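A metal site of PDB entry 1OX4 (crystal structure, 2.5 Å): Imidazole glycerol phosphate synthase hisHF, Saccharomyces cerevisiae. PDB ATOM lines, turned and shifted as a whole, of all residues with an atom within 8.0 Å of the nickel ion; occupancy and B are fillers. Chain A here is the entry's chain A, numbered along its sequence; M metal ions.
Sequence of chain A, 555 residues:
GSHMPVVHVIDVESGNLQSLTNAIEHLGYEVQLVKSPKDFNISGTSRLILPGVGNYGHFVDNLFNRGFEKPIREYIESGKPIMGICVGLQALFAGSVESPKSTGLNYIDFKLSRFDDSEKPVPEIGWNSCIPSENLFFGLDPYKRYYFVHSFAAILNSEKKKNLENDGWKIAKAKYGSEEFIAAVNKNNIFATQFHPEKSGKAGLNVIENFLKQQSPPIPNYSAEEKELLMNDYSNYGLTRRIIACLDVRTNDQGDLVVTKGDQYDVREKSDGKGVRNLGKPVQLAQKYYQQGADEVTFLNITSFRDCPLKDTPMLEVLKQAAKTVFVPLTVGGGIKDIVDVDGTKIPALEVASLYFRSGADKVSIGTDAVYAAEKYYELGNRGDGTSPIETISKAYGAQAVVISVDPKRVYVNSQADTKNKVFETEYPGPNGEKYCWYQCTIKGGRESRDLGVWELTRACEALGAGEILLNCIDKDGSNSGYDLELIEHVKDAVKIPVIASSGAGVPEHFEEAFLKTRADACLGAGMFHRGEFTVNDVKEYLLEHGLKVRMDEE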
ATOM      1  N   GLY A   1       4.990 -26.896  16.390  1.00  0.00           N
ATOM      2  CA  GLY A   1       5.604 -27.280  15.130  1.00  0.00           C
ATOM      3  C   GLY A   1       7.089 -26.991  15.130  1.00  0.00           C
ATOM      4  O   GLY A   1       7.843 -27.518  14.311  1.00  0.00           O
ATOM      5  N   SER A   2       7.494 -26.127  16.054  1.00  0.00           N
ATOM      6  CA  SER A   2       8.885 -25.733  16.245  1.00  0.00           C
ATOM      7  C   SER A   2       8.992 -25.007  17.560  1.00  0.00           C
ATOM      8  O   SER A   2      10.086 -24.658  18.020  1.00  0.00           O
ATOM      9  CB  SER A   2       9.363 -24.828  15.099  1.00  0.00           C
ATOM     10  OG  SER A   2       8.507 -23.716  14.935  1.00  0.00           O
ATOM     11  N   HIS A   3       7.828 -24.759  18.185  1.00  0.00           N
ATOM     12  CA  HIS A   3       7.856 -24.005  19.440  1.00  0.00           C
ATOM     13  C   HIS A   3       8.325 -24.904  20.593  1.00  0.00           C
ATOM     14  O   HIS A   3       8.497 -24.438  21.718  1.00  0.00           O
ATOM     15  CB  HIS A   3       6.503 -23.388  19.794  1.00  0.00           C
ATOM     16  CG  HIS A   3       5.352 -24.395  20.015  1.00  0.00           C
ATOM     17  ND1 HIS A   3       5.046 -25.397  19.129  1.00  0.00           N
ATOM     18  CD2 HIS A   3       4.451 -24.497  21.024  1.00  0.00           C
ATOM     19  CE1 HIS A   3       4.019 -26.089  19.578  1.00  0.00           C
ATOM     20  NE2 HIS A   3       3.640 -25.560  20.735  1.00  0.00           N
ATOM     21  N   MET A   4       8.563 -26.189  20.305  1.00  0.00           N
ATOM     22  CA  MET A   4       9.089 -27.151  21.286  1.00  0.00           C
ATOM     23  C   MET A   4       9.761 -28.300  20.523  1.00  0.00           C
ATOM     24  O   MET A   4       9.397 -28.584  19.387  1.00  0.00           O
ATOM     25  CB  MET A   4       8.002 -27.687  22.216  1.00  0.00           C
ATOM     26  CG  MET A   4       6.730 -28.232  21.552  1.00  0.00           C
ATOM     27  SD  MET A   4       5.544 -28.855  22.750  1.00  0.00           S
ATOM     28  CE  MET A   4       4.772 -27.337  23.308  1.00  0.00           C
ATOM     29  N   PRO A   5      10.747 -28.964  21.140  1.00  0.00           N
ATOM     30  CA  PRO A   5      11.441 -30.063  20.450  1.00  0.00           C
ATOM     31  C   PRO A   5      10.412 -31.078  19.987  1.00  0.00           C
ATOM     32  O   PRO A   5       9.419 -31.332  20.692  1.00  0.00           O
ATOM     33  CB  PRO A   5      12.346 -30.647  21.528  1.00  0.00           C
ATOM     34  CG  PRO A   5      12.484 -29.553  22.545  1.00  0.00           C
ATOM     35  CD  PRO A   5      11.123 -28.917  22.562  1.00  0.00           C
ATOM     36  N   VAL A   6      10.614 -31.682  18.825  1.00  0.00           N
ATOM     37  CA  VAL A   6       9.600 -32.624  18.433  1.00  0.00           C
ATOM     38  C   VAL A   6      10.124 -34.043  18.508  1.00  0.00           C
ATOM     39  O   VAL A   6      11.272 -34.320  18.149  1.00  0.00           O
ATOM     40  CB  VAL A   6       9.052 -32.348  17.034  1.00  0.00           C
ATOM     41  CG1 VAL A   6       8.053 -33.437  16.654  1.00  0.00           C
ATOM     42  CG2 VAL A   6       8.388 -30.975  17.000  1.00  0.00           C
ATOM     43  N   GLU A  30       6.546 -32.212  22.003  1.00  0.00           N
ATOM     44  CA  GLU A  30       5.425 -32.351  21.112  1.00  0.00           C
ATOM     45  C   GLU A  30       5.608 -33.685  20.442  1.00  0.00           C
ATOM     46  O   GLU A  30       6.712 -34.009  20.002  1.00  0.00           O
ATOM     47  CB  GLU A  30       5.402 -31.251  20.041  1.00  0.00           C
ATOM     48  CG  GLU A  30       4.217 -31.358  19.097  1.00  0.00           C
ATOM     49  CD  GLU A  30       4.181 -30.265  18.044  1.00  0.00           C
ATOM     50  OE1 GLU A  30       4.060 -29.077  18.424  1.00  0.00           O
ATOM     51  OE2 GLU A  30       4.284 -30.579  16.838  1.00  0.00           O
HETATM   52 NI    NI M   1       6.218 -25.735  17.527  1.00  0.00          NI
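The side-chain carboxylate of Glu 30 lies close to the backbone NH of Gly 1 (3.1 Å).
The side-chain sulfur (SD) of Met 4 sits at hydrogen-bond distance from the backbone NH (N) of Glu 30.
Merely in contact with the nickel ion: Met 4 (3.7 Å).
Of the 7 residues printed, 4 come within 4 Å of the nickel ion.
The nearest printed residue that does not touch the nickel ion is Glu 30 (4.1 Å).
The backbone nitrogen (N) of Ser 2 is bound to the nickel ion (2.0 Å).
N of His 3 binds the nickel ion.
ND1 of His 3 binds the nickel ion (2.0 Å).
N of Gly 1 binds the nickel ion (2.0 Å).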
